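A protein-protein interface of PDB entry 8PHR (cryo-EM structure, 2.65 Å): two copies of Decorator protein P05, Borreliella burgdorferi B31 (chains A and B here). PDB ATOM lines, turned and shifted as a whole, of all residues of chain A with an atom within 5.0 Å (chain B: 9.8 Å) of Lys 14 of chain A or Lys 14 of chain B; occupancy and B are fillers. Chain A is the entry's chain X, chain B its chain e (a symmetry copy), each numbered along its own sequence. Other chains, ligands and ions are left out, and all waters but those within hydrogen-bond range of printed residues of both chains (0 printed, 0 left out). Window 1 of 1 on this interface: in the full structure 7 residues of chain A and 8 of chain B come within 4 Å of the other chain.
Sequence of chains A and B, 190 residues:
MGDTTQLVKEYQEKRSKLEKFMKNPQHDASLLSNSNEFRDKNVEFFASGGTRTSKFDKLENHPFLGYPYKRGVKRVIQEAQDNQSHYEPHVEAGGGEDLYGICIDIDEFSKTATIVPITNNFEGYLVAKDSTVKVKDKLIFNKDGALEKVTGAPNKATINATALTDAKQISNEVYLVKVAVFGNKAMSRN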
ATOM      1  N   GLU A  10      -1.785  11.616 -14.246  1.00  0.00           N
ATOM      2  CA  GLU A  10      -2.566  10.865 -13.268  1.00  0.00           C
ATOM      3  C   GLU A  10      -3.814  10.271 -13.905  1.00  0.00           C
ATOM      4  O   GLU A  10      -4.215   9.150 -13.575  1.00  0.00           O
ATOM      5  CB  GLU A  10      -2.940  11.762 -12.087  1.00  0.00           C
ATOM      6  CG  GLU A  10      -1.762  12.193 -11.229  1.00  0.00           C
ATOM      7  CD  GLU A  10      -2.092  13.379 -10.342  1.00  0.00           C
ATOM      8  OE1 GLU A  10      -3.235  13.876 -10.411  1.00  0.00           O
ATOM      9  OE2 GLU A  10      -1.206  13.813  -9.575  1.00  0.00           O
ATOM     10  N   TYR A  11      -4.444  11.014 -14.818  1.00  0.00           N
ATOM     11  CA  TYR A  11      -5.593  10.482 -15.541  1.00  0.00           C
ATOM     12  C   TYR A  11      -5.211   9.246 -16.345  1.00  0.00           C
ATOM     13  O   TYR A  11      -5.941   8.248 -16.342  1.00  0.00           O
ATOM     14  CB  TYR A  11      -6.180  11.556 -16.457  1.00  0.00           C
ATOM     15  CG  TYR A  11      -7.381  11.096 -17.252  1.00  0.00           C
ATOM     16  CD1 TYR A  11      -8.620  10.930 -16.647  1.00  0.00           C
ATOM     17  CD2 TYR A  11      -7.275  10.825 -18.610  1.00  0.00           C
ATOM     18  CE1 TYR A  11      -9.719  10.509 -17.372  1.00  0.00           C
ATOM     19  CE2 TYR A  11      -8.367  10.403 -19.343  1.00  0.00           C
ATOM     20  CZ  TYR A  11      -9.587  10.247 -18.719  1.00  0.00           C
ATOM     21  OH  TYR A  11     -10.676   9.827 -19.446  1.00  0.00           O
ATOM     22  N   GLN A  12      -4.072   9.294 -17.040  1.00  0.00           N
ATOM     23  CA  GLN A  12      -3.625   8.128 -17.800  1.00  0.00           C
ATOM     24  C   GLN A  12      -3.379   6.936 -16.882  1.00  0.00           C
ATOM     25  O   GLN A  12      -3.788   5.809 -17.188  1.00  0.00           O
ATOM     26  CB  GLN A  12      -2.360   8.449 -18.598  1.00  0.00           C
ATOM     27  CG  GLN A  12      -2.427   9.700 -19.449  1.00  0.00           C
ATOM     28  CD  GLN A  12      -1.065  10.337 -19.642  1.00  0.00           C
ATOM     29  OE1 GLN A  12      -0.055   9.825 -19.160  1.00  0.00           O
ATOM     30  NE2 GLN A  12      -1.030  11.454 -20.358  1.00  0.00           N
ATOM     31  N   GLU A  13      -2.705   7.166 -15.752  1.00  0.00           N
ATOM     32  CA  GLU A  13      -2.419   6.067 -14.831  1.00  0.00           C
ATOM     33  C   GLU A  13      -3.703   5.449 -14.289  1.00  0.00           C
ATOM     34  O   GLU A  13      -3.854   4.221 -14.265  1.00  0.00           O
ATOM     35  CB  GLU A  13      -1.528   6.546 -13.683  1.00  0.00           C
ATOM     36  CG  GLU A  13      -0.260   7.257 -14.117  1.00  0.00           C
ATOM     37  CD  GLU A  13       0.316   8.136 -13.024  1.00  0.00           C
ATOM     38  OE1 GLU A  13      -0.249   8.148 -11.909  1.00  0.00           O
ATOM     39  OE2 GLU A  13       1.334   8.814 -13.278  1.00  0.00           O
ATOM     40  N   LYS A  14      -4.644   6.289 -13.849  1.00  0.00           N
ATOM     41  CA  LYS A  14      -5.894   5.774 -13.300  1.00  0.00           C
ATOM     42  C   LYS A  14      -6.705   5.042 -14.360  1.00  0.00           C
ATOM     43  O   LYS A  14      -7.295   3.992 -14.082  1.00  0.00           O
ATOM     44  CB  LYS A  14      -6.711   6.909 -12.682  1.00  0.00           C
ATOM     45  CG  LYS A  14      -6.030   7.628 -11.522  1.00  0.00           C
ATOM     46  CD  LYS A  14      -6.025   6.795 -10.246  1.00  0.00           C
ATOM     47  CE  LYS A  14      -4.672   6.142  -9.998  1.00  0.00           C
ATOM     48  NZ  LYS A  14      -4.637   5.412  -8.700  1.00  0.00           N
ATOM     49  N   ARG A  15      -6.750   5.578 -15.583  1.00  0.00           N
ATOM     50  CA  ARG A  15      -7.489   4.914 -16.650  1.00  0.00           C
ATOM     51  C   ARG A  15      -6.875   3.562 -16.984  1.00  0.00           C
ATOM     52  O   ARG A  15      -7.598   2.581 -17.194  1.00  0.00           O
ATOM     53  CB  ARG A  15      -7.537   5.802 -17.893  1.00  0.00           C
ATOM     54  CG  ARG A  15      -8.373   5.221 -19.021  1.00  0.00           C
ATOM     55  CD  ARG A  15      -8.276   6.059 -20.283  1.00  0.00           C
ATOM     56  NE  ARG A  15      -9.100   5.514 -21.355  1.00  0.00           N
ATOM     57  CZ  ARG A  15      -9.196   6.038 -22.569  1.00  0.00           C
ATOM     58  NH1 ARG A  15      -8.531   7.131 -22.905  1.00  0.00           N
ATOM     59  NH2 ARG A  15      -9.977   5.449 -23.469  1.00  0.00           N
ATOM     60  N   SER A  16      -5.542   3.487 -17.038  1.00  0.00           N
ATOM     61  CA  SER A  16      -4.889   2.210 -17.308  1.00  0.00           C
ATOM     62  C   SER A  16      -5.170   1.202 -16.200  1.00  0.00           C
ATOM     63  O   SER A  16      -5.490   0.038 -16.475  1.00  0.00           O
ATOM     64  CB  SER A  16      -3.385   2.415 -17.482  1.00  0.00           C
ATOM     65  OG  SER A  16      -2.807   2.969 -16.312  1.00  0.00           O
ATOM     66  N   LYS A  17      -5.071   1.635 -14.939  1.00  0.00           N
ATOM     67  CA  LYS A  17      -5.343   0.724 -13.830  1.00  0.00           C
ATOM     68  C   LYS A  17      -6.785   0.234 -13.857  1.00  0.00           C
ATOM     69  O   LYS A  17      -7.050  -0.950 -13.615  1.00  0.00           O
ATOM     70  CB  LYS A  17      -5.035   1.405 -12.496  1.00  0.00           C
ATOM     71  CG  LYS A  17      -3.564   1.726 -12.278  1.00  0.00           C
ATOM     72  CD  LYS A  17      -3.371   2.610 -11.057  1.00  0.00           C
ATOM     73  CE  LYS A  17      -1.900   2.902 -10.809  1.00  0.00           C
ATOM     74  NZ  LYS A  17      -1.232   3.470 -12.013  1.00  0.00           N
ATOM     75  N   LEU A  18      -7.731   1.129 -14.149  1.00  0.00           N
ATOM     76  CA  LEU A  18      -9.136   0.740 -14.181  1.00  0.00           C
ATOM     77  C   LEU A  18      -9.424  -0.211 -15.337  1.00  0.00           C
ATOM     78  O   LEU A  18     -10.111  -1.224 -15.164  1.00  0.00           O
ATOM     79  CB  LEU A  18     -10.019   1.984 -14.271  1.00  0.00           C
ATOM     80  CG  LEU A  18     -11.518   1.708 -14.348  1.00  0.00           C
ATOM     81  CD1 LEU A  18     -12.005   1.158 -13.022  1.00  0.00           C
ATOM     82  CD2 LEU A  18     -12.279   2.971 -14.720  1.00  0.00           C
ATOM     83  N   GLU A  19      -8.906   0.098 -16.528  1.00  0.00           N
ATOM     84  CA  GLU A  19      -9.144  -0.738 -17.697  1.00  0.00           C
ATOM     85  C   GLU A  19      -8.366  -2.045 -17.657  1.00  0.00           C
ATOM     86  O   GLU A  19      -8.662  -2.943 -18.453  1.00  0.00           O
ATOM     87  CB  GLU A  19      -8.802   0.043 -18.967  1.00  0.00           C
ATOM     88  CG  GLU A  19      -9.964   0.864 -19.508  1.00  0.00           C
ATOM     89  CD  GLU A  19      -9.517   1.978 -20.432  1.00  0.00           C
ATOM     90  OE1 GLU A  19      -8.297   2.233 -20.511  1.00  0.00           O
ATOM     91  OE2 GLU A  19     -10.386   2.598 -21.081  1.00  0.00           O
ATOM     92  N   THR B   4     -11.646  -2.304  -7.674  1.00  0.00           N
ATOM     93  CA  THR B   4     -12.471  -1.975  -8.832  1.00  0.00           C
ATOM     94  C   THR B   4     -13.286  -0.712  -8.579  1.00  0.00           C
ATOM     95  O   THR B   4     -13.115   0.292  -9.270  1.00  0.00           O
ATOM     96  CB  THR B   4     -13.424  -3.132  -9.191  1.00  0.00           C
ATOM     97  OG1 THR B   4     -12.662  -4.313  -9.468  1.00  0.00           O
ATOM     98  CG2 THR B   4     -14.257  -2.774 -10.412  1.00  0.00           C
ATOM     99  N   GLN B   6     -13.085   1.246  -5.969  1.00  0.00           N
ATOM    100  CA  GLN B   6     -12.151   2.283  -5.543  1.00  0.00           C
ATOM    101  C   GLN B   6     -11.441   2.904  -6.741  1.00  0.00           C
ATOM    102  O   GLN B   6     -11.227   4.121  -6.786  1.00  0.00           O
ATOM    103  CB  GLN B   6     -11.134   1.704  -4.558  1.00  0.00           C
ATOM    104  CG  GLN B   6     -11.746   0.887  -3.430  1.00  0.00           C
ATOM    105  CD  GLN B   6     -10.696   0.197  -2.579  1.00  0.00           C
ATOM    106  OE1 GLN B   6      -9.496   0.356  -2.803  1.00  0.00           O
ATOM    107  NE2 GLN B   6     -11.144  -0.575  -1.596  1.00  0.00           N
ATOM    108  N   LEU B   7     -11.067   2.077  -7.719  1.00  0.00           N
ATOM    109  CA  LEU B   7     -10.451   2.595  -8.937  1.00  0.00           C
ATOM    110  C   LEU B   7     -11.416   3.492  -9.703  1.00  0.00           C
ATOM    111  O   LEU B   7     -11.009   4.514 -10.265  1.00  0.00           O
ATOM    112  CB  LEU B   7      -9.969   1.441  -9.816  1.00  0.00           C
ATOM    113  CG  LEU B   7      -8.582   0.856  -9.529  1.00  0.00           C
ATOM    114  CD1 LEU B   7      -8.525   0.168  -8.171  1.00  0.00           C
ATOM    115  CD2 LEU B   7      -8.176  -0.110 -10.628  1.00  0.00           C
ATOM    116  N   VAL B   8     -12.700   3.125  -9.736  1.00  0.00           N
ATOM    117  CA  VAL B   8     -13.701   3.972 -10.380  1.00  0.00           C
ATOM    118  C   VAL B   8     -13.799   5.316  -9.668  1.00  0.00           C
ATOM    119  O   VAL B   8     -13.888   6.371 -10.307  1.00  0.00           O
ATOM    120  CB  VAL B   8     -15.067   3.258 -10.427  1.00  0.00           C
ATOM    121  CG1 VAL B   8     -16.122   4.164 -11.039  1.00  0.00           C
ATOM    122  CG2 VAL B   8     -14.970   1.966 -11.217  1.00  0.00           C
ATOM    123  N   LYS B   9     -13.796   5.296  -8.332  1.00  0.00           N
ATOM    124  CA  LYS B   9     -13.855   6.547  -7.577  1.00  0.00           C
ATOM    125  C   LYS B   9     -12.637   7.421  -7.855  1.00  0.00           C
ATOM    126  O   LYS B   9     -12.766   8.640  -8.038  1.00  0.00           O
ATOM    127  CB  LYS B   9     -13.975   6.256  -6.080  1.00  0.00           C
ATOM    128  CG  LYS B   9     -15.172   5.401  -5.707  1.00  0.00           C
ATOM    129  CD  LYS B   9     -14.941   4.678  -4.390  1.00  0.00           C
ATOM    130  CE  LYS B   9     -15.998   3.613  -4.153  1.00  0.00           C
ATOM    131  NZ  LYS B   9     -15.698   2.797  -2.944  1.00  0.00           N
ATOM    132  N   GLU B  10     -11.445   6.819  -7.891  1.00  0.00           N
ATOM    133  CA  GLU B  10     -10.243   7.586  -8.208  1.00  0.00           C
ATOM    134  C   GLU B  10     -10.312   8.161  -9.619  1.00  0.00           C
ATOM    135  O   GLU B  10      -9.896   9.302  -9.855  1.00  0.00           O
ATOM    136  CB  GLU B  10      -8.996   6.715  -8.045  1.00  0.00           C
ATOM    137  CG  GLU B  10      -8.804   6.150  -6.649  1.00  0.00           C
ATOM    138  CD  GLU B  10      -8.006   4.861  -6.648  1.00  0.00           C
ATOM    139  OE1 GLU B  10      -7.560   4.435  -7.734  1.00  0.00           O
ATOM    140  OE2 GLU B  10      -7.826   4.272  -5.561  1.00  0.00           O
ATOM    141  N   TYR B  11     -10.827   7.377 -10.569  1.00  0.00           N
ATOM    142  CA  TYR B  11     -10.997   7.873 -11.929  1.00  0.00           C
ATOM    143  C   TYR B  11     -11.939   9.067 -11.960  1.00  0.00           C
ATOM    144  O   TYR B  11     -11.682  10.049 -12.662  1.00  0.00           O
ATOM    145  CB  TYR B  11     -11.515   6.756 -12.838  1.00  0.00           C
ATOM    146  CG  TYR B  11     -12.249   7.253 -14.064  1.00  0.00           C
ATOM    147  CD1 TYR B  11     -11.571   7.890 -15.094  1.00  0.00           C
ATOM    148  CD2 TYR B  11     -13.622   7.089 -14.186  1.00  0.00           C
ATOM    149  CE1 TYR B  11     -12.240   8.344 -16.217  1.00  0.00           C
ATOM    150  CE2 TYR B  11     -14.301   7.541 -15.304  1.00  0.00           C
ATOM    151  CZ  TYR B  11     -13.604   8.169 -16.315  1.00  0.00           C
ATOM    152  OH  TYR B  11     -14.275   8.620 -17.428  1.00  0.00           O
ATOM    153  N   GLN B  12     -13.037   9.001 -11.202  1.00  0.00           N
ATOM    154  CA  GLN B  12     -13.953  10.137 -11.132  1.00  0.00           C
ATOM    155  C   GLN B  12     -13.273  11.364 -10.540  1.00  0.00           C
ATOM    156  O   GLN B  12     -13.468  12.485 -11.025  1.00  0.00           O
ATOM    157  CB  GLN B  12     -15.197   9.778 -10.319  1.00  0.00           C
ATOM    158  CG  GLN B  12     -16.000   8.614 -10.866  1.00  0.00           C
ATOM    159  CD  GLN B  12     -16.860   7.957  -9.805  1.00  0.00           C
ATOM    160  OE1 GLN B  12     -16.814   8.334  -8.633  1.00  0.00           O
ATOM    161  NE2 GLN B  12     -17.658   6.977 -10.210  1.00  0.00           N
ATOM    162  N   GLU B  13     -12.477  11.177  -9.482  1.00  0.00           N
ATOM    163  CA  GLU B  13     -11.789  12.312  -8.869  1.00  0.00           C
ATOM    164  C   GLU B  13     -10.828  12.973  -9.852  1.00  0.00           C
ATOM    165  O   GLU B  13     -10.832  14.202 -10.014  1.00  0.00           O
ATOM    166  CB  GLU B  13     -11.047  11.867  -7.608  1.00  0.00           C
ATOM    167  CG  GLU B  13     -11.927  11.212  -6.557  1.00  0.00           C
ATOM    168  CD  GLU B  13     -11.147  10.293  -5.636  1.00  0.00           C
ATOM    169  OE1 GLU B  13      -9.913  10.197  -5.795  1.00  0.00           O
ATOM    170  OE2 GLU B  13     -11.770   9.668  -4.752  1.00  0.00           O
ATOM    171  N   LYS B  14      -9.995  12.173 -10.523  1.00  0.00           N
ATOM    172  CA  LYS B  14      -9.054  12.748 -11.483  1.00  0.00           C
ATOM    173  C   LYS B  14      -9.772  13.357 -12.682  1.00  0.00           C
ATOM    174  O   LYS B  14      -9.326  14.378 -13.216  1.00  0.00           O
ATOM    175  CB  LYS B  14      -8.036  11.702 -11.942  1.00  0.00           C
ATOM    176  CG  LYS B  14      -7.435  10.862 -10.827  1.00  0.00           C
ATOM    177  CD  LYS B  14      -6.943  11.725  -9.673  1.00  0.00           C
ATOM    178  CE  LYS B  14      -6.862  10.927  -8.381  1.00  0.00           C
ATOM    179  NZ  LYS B  14      -6.559  11.797  -7.211  1.00  0.00           N
ATOM    180  N   ARG B  15     -10.883  12.754 -13.114  1.00  0.00           N
ATOM    181  CA  ARG B  15     -11.656  13.325 -14.208  1.00  0.00           C
ATOM    182  C   ARG B  15     -12.236  14.677 -13.822  1.00  0.00           C
ATOM    183  O   ARG B  15     -12.241  15.611 -14.630  1.00  0.00           O
ATOM    184  CB  ARG B  15     -12.765  12.358 -14.624  1.00  0.00           C
ATOM    185  CG  ARG B  15     -13.617  12.843 -15.784  1.00  0.00           C
ATOM    186  CD  ARG B  15     -14.798  11.917 -16.025  1.00  0.00           C
ATOM    187  NE  ARG B  15     -15.628  12.366 -17.135  1.00  0.00           N
ATOM    188  CZ  ARG B  15     -16.714  11.734 -17.562  1.00  0.00           C
ATOM    189  NH1 ARG B  15     -17.132  10.617 -16.991  1.00  0.00           N
ATOM    190  NH2 ARG B  15     -17.397  12.237 -18.587  1.00  0.00           N
ATOM    191  N   SER B  16     -12.731  14.803 -12.588  1.00  0.00           N
ATOM    192  CA  SER B  16     -13.236  16.091 -12.122  1.00  0.00           C
ATOM    193  C   SER B  16     -12.120  17.126 -12.047  1.00  0.00           C
ATOM    194  O   SER B  16     -12.307  18.282 -12.447  1.00  0.00           O
ATOM    195  CB  SER B  16     -13.910  15.926 -10.760  1.00  0.00           C
ATOM    196  OG  SER B  16     -12.997  15.432  -9.796  1.00  0.00           O
ATOM    197  N   LYS B  17     -10.947  16.727 -11.543  1.00  0.00           N
ATOM    198  CA  LYS B  17      -9.826  17.661 -11.480  1.00  0.00           C
ATOM    199  C   LYS B  17      -9.421  18.135 -12.873  1.00  0.00           C
ATOM    200  O   LYS B  17      -9.151  19.325 -13.077  1.00  0.00           O
ATOM    201  CB  LYS B  17      -8.634  17.026 -10.764  1.00  0.00           C
ATOM    202  CG  LYS B  17      -8.907  16.610  -9.328  1.00  0.00           C
ATOM    203  CD  LYS B  17      -7.661  16.019  -8.686  1.00  0.00           C
ATOM    204  CE  LYS B  17      -7.935  15.538  -7.271  1.00  0.00           C
ATOM    205  NZ  LYS B  17      -8.910  14.414  -7.244  1.00  0.00           N
ATOM    206  N   LEU B  18      -9.366  17.218 -13.842  1.00  0.00           N
ATOM    207  CA  LEU B  18      -9.012  17.605 -15.204  1.00  0.00           C
ATOM    208  C   LEU B  18     -10.089  18.483 -15.833  1.00  0.00           C
ATOM    209  O   LEU B  18      -9.777  19.472 -16.506  1.00  0.00           O
ATOM    210  CB  LEU B  18      -8.771  16.360 -16.057  1.00  0.00           C
ATOM    211  CG  LEU B  18      -8.584  16.594 -17.558  1.00  0.00           C
ATOM    212  CD1 LEU B  18      -7.211  17.183 -17.842  1.00  0.00           C
ATOM    213  CD2 LEU B  18      -8.790  15.304 -18.335  1.00  0.00           C
ATOM    214  N   GLU B  19     -11.363  18.139 -15.623  1.00  0.00           N
ATOM    215  CA  GLU B  19     -12.465  18.900 -16.197  1.00  0.00           C
ATOM    216  C   GLU B  19     -12.597  20.283 -15.578  1.00  0.00           C
ATOM    217  O   GLU B  19     -13.192  21.170 -16.199  1.00  0.00           O
ATOM    218  CB  GLU B  19     -13.771  18.123 -16.029  1.00  0.00           C
ATOM    219  CG  GLU B  19     -14.016  17.083 -17.111  1.00  0.00           C
ATOM    220  CD  GLU B  19     -15.059  16.059 -16.710  1.00  0.00           C
ATOM    221  OE1 GLU B  19     -15.458  16.048 -15.527  1.00  0.00           O
ATOM    222  OE2 GLU B  19     -15.477  15.264 -17.577  1.00  0.00           O
ATOM    223  N   LYS B  20     -12.071  20.481 -14.367  1.00  0.00           N
ATOM    224  CA  LYS B  20     -12.070  21.816 -13.779  1.00  0.00           C
ATOM    225  C   LYS B  20     -11.282  22.794 -14.643  1.00  0.00           C
ATOM    226  O   LYS B  20     -11.693  23.946 -14.822  1.00  0.00           O
ATOM    227  CB  LYS B  20     -11.500  21.764 -12.360  1.00  0.00           C
ATOM    228  CG  LYS B  20     -11.736  23.023 -11.534  1.00  0.00           C
ATOM    229  CD  LYS B  20     -10.555  23.980 -11.621  1.00  0.00           C
ATOM    230  CE  LYS B  20     -10.660  25.091 -10.592  1.00  0.00           C
ATOM    231  NZ  LYS B  20      -9.482  26.000 -10.648  1.00  0.00           N
ATOM    232  N   PHE B  21     -10.148  22.354 -15.184  1.00  0.00           N
ATOM    233  CA  PHE B  21      -9.327  23.191 -16.056  1.00  0.00           C
ATOM    234  C   PHE B  21      -9.675  22.908 -17.517  1.00  0.00           C
ATOM    235  O   PHE B  21      -8.873  22.397 -18.301  1.00  0.00           O
ATOM    236  CB  PHE B  21      -7.846  22.953 -15.777  1.00  0.00           C
ATOM    237  CG  PHE B  21      -7.410  23.376 -14.404  1.00  0.00           C
ATOM    238  CD1 PHE B  21      -7.150  24.708 -14.123  1.00  0.00           C
ATOM    239  CD2 PHE B  21      -7.255  22.440 -13.395  1.00  0.00           C
ATOM    240  CE1 PHE B  21      -6.748  25.098 -12.860  1.00  0.00           C
ATOM    241  CE2 PHE B  21      -6.853  22.825 -12.129  1.00  0.00           C
ATOM    242  CZ  PHE B  21      -6.598  24.156 -11.861  1.00  0.00           C
ATOM    243  N   MET B  22     -10.908  23.260 -17.876  1.00  0.00           N
ATOM    244  CA  MET B  22     -11.391  23.064 -19.235  1.00  0.00           C
ATOM    245  C   MET B  22     -12.410  24.145 -19.565  1.00  0.00           C
ATOM    246  O   MET B  22     -13.182  24.574 -18.704  1.00  0.00           O
ATOM    247  CB  MET B  22     -12.016  21.676 -19.421  1.00  0.00           C
ATOM    248  CG  MET B  22     -11.073  20.647 -20.023  1.00  0.00           C
ATOM    249  SD  MET B  22     -11.815  19.007 -20.134  1.00  0.00           S
ATOM    250  CE  MET B  22     -12.586  19.095 -21.748  1.00  0.00           C
ATOM    251  N   HIS B  27     -19.994  16.721 -19.884  1.00  0.00           N
ATOM    252  CA  HIS B  27     -20.568  15.950 -18.793  1.00  0.00           C
ATOM    253  C   HIS B  27     -21.921  15.395 -19.212  1.00  0.00           C
ATOM    254  O   HIS B  27     -22.637  15.999 -20.014  1.00  0.00           O
ATOM    255  CB  HIS B  27     -20.746  16.792 -17.514  1.00  0.00           C
ATOM    256  CG  HIS B  27     -19.471  17.358 -16.970  1.00  0.00           C
ATOM    257  ND1 HIS B  27     -19.103  17.220 -15.650  1.00  0.00           N
ATOM    258  CD2 HIS B  27     -18.486  18.077 -17.560  1.00  0.00           C
ATOM    259  CE1 HIS B  27     -17.944  17.820 -15.451  1.00  0.00           C
ATOM    260  NE2 HIS B  27     -17.548  18.349 -16.594  1.00  0.00           N
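The side-chain amino group of Lys 14 of chain A is in salt-bridge range of the side-chain carboxylate of Glu 10 of chain B (3.2 Å).
OE1 of Glu 13 of chain B is in salt-bridge range of NZ of Lys 14 of chain B, 3.98 Å away.
Among the printed residues, pairs that only touch across the chains: Tyr 11 of chain A with Tyr 11 of chain B, Lys 14 of chain A with Lys 14 of chain B, Lys 17 of chain A with Leu 7 of chain B, Leu 18 of chain A with Leu 7 of chain B and Leu 18 of chain A with Val 8 of chain B.
Of chain B, only Glu 10 (3.2 Å) and Lys 14 (3.6 Å) come within 4 Å of Lys 14 of chain A.
No residue of chain B comes within 4 Å of Ser 16 of chain A.
Of chain B, only Leu 7 (3.3 Å) comes within 4 Å of Lys 17 of chain A.
Of the printed residues of chain B, Leu 18 of chain A touches Leu 7 and Val 8.
Of the printed residues of chain A, Tyr 11 of chain B touches Tyr 11.
Of the printed residues of chain B, Tyr 11 of chain A touches Tyr 11.
Glu 10 of chain A touches none of the printed residues of chain B.
Ser 16 of chain B touches none of the printed residues of chain A.
The nearest residue of chain B that does not touch Lys 14 of chain A is Tyr 11 of chain B (4.5 Å).
The nearest residue of chain A that does not touch Lys 14 of chain B is Glu 10 of chain A (4.3 Å).
Of the 19 printed residues of chain B, 5 touch a printed residue of chain A.
Tyr 11 of chain A touches its own counterpart, Tyr 11 of chain B.
Lys 14 of chain A touches Glu 10 of chain B, but with the chains exchanged Glu 10 of chain A does not touch Lys 14 of chain B (4.3 Å).
Lys 14 of chain A touches its own counterpart, Lys 14 of chain B.
Positions printed for both chains: 10, 11, 12, 13, 14, 15, 16, 17, 18 and 19.
Of the 6 pairs that touch across the chains among the printed residues, 2 have their exchanged pair printed and touching as well.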
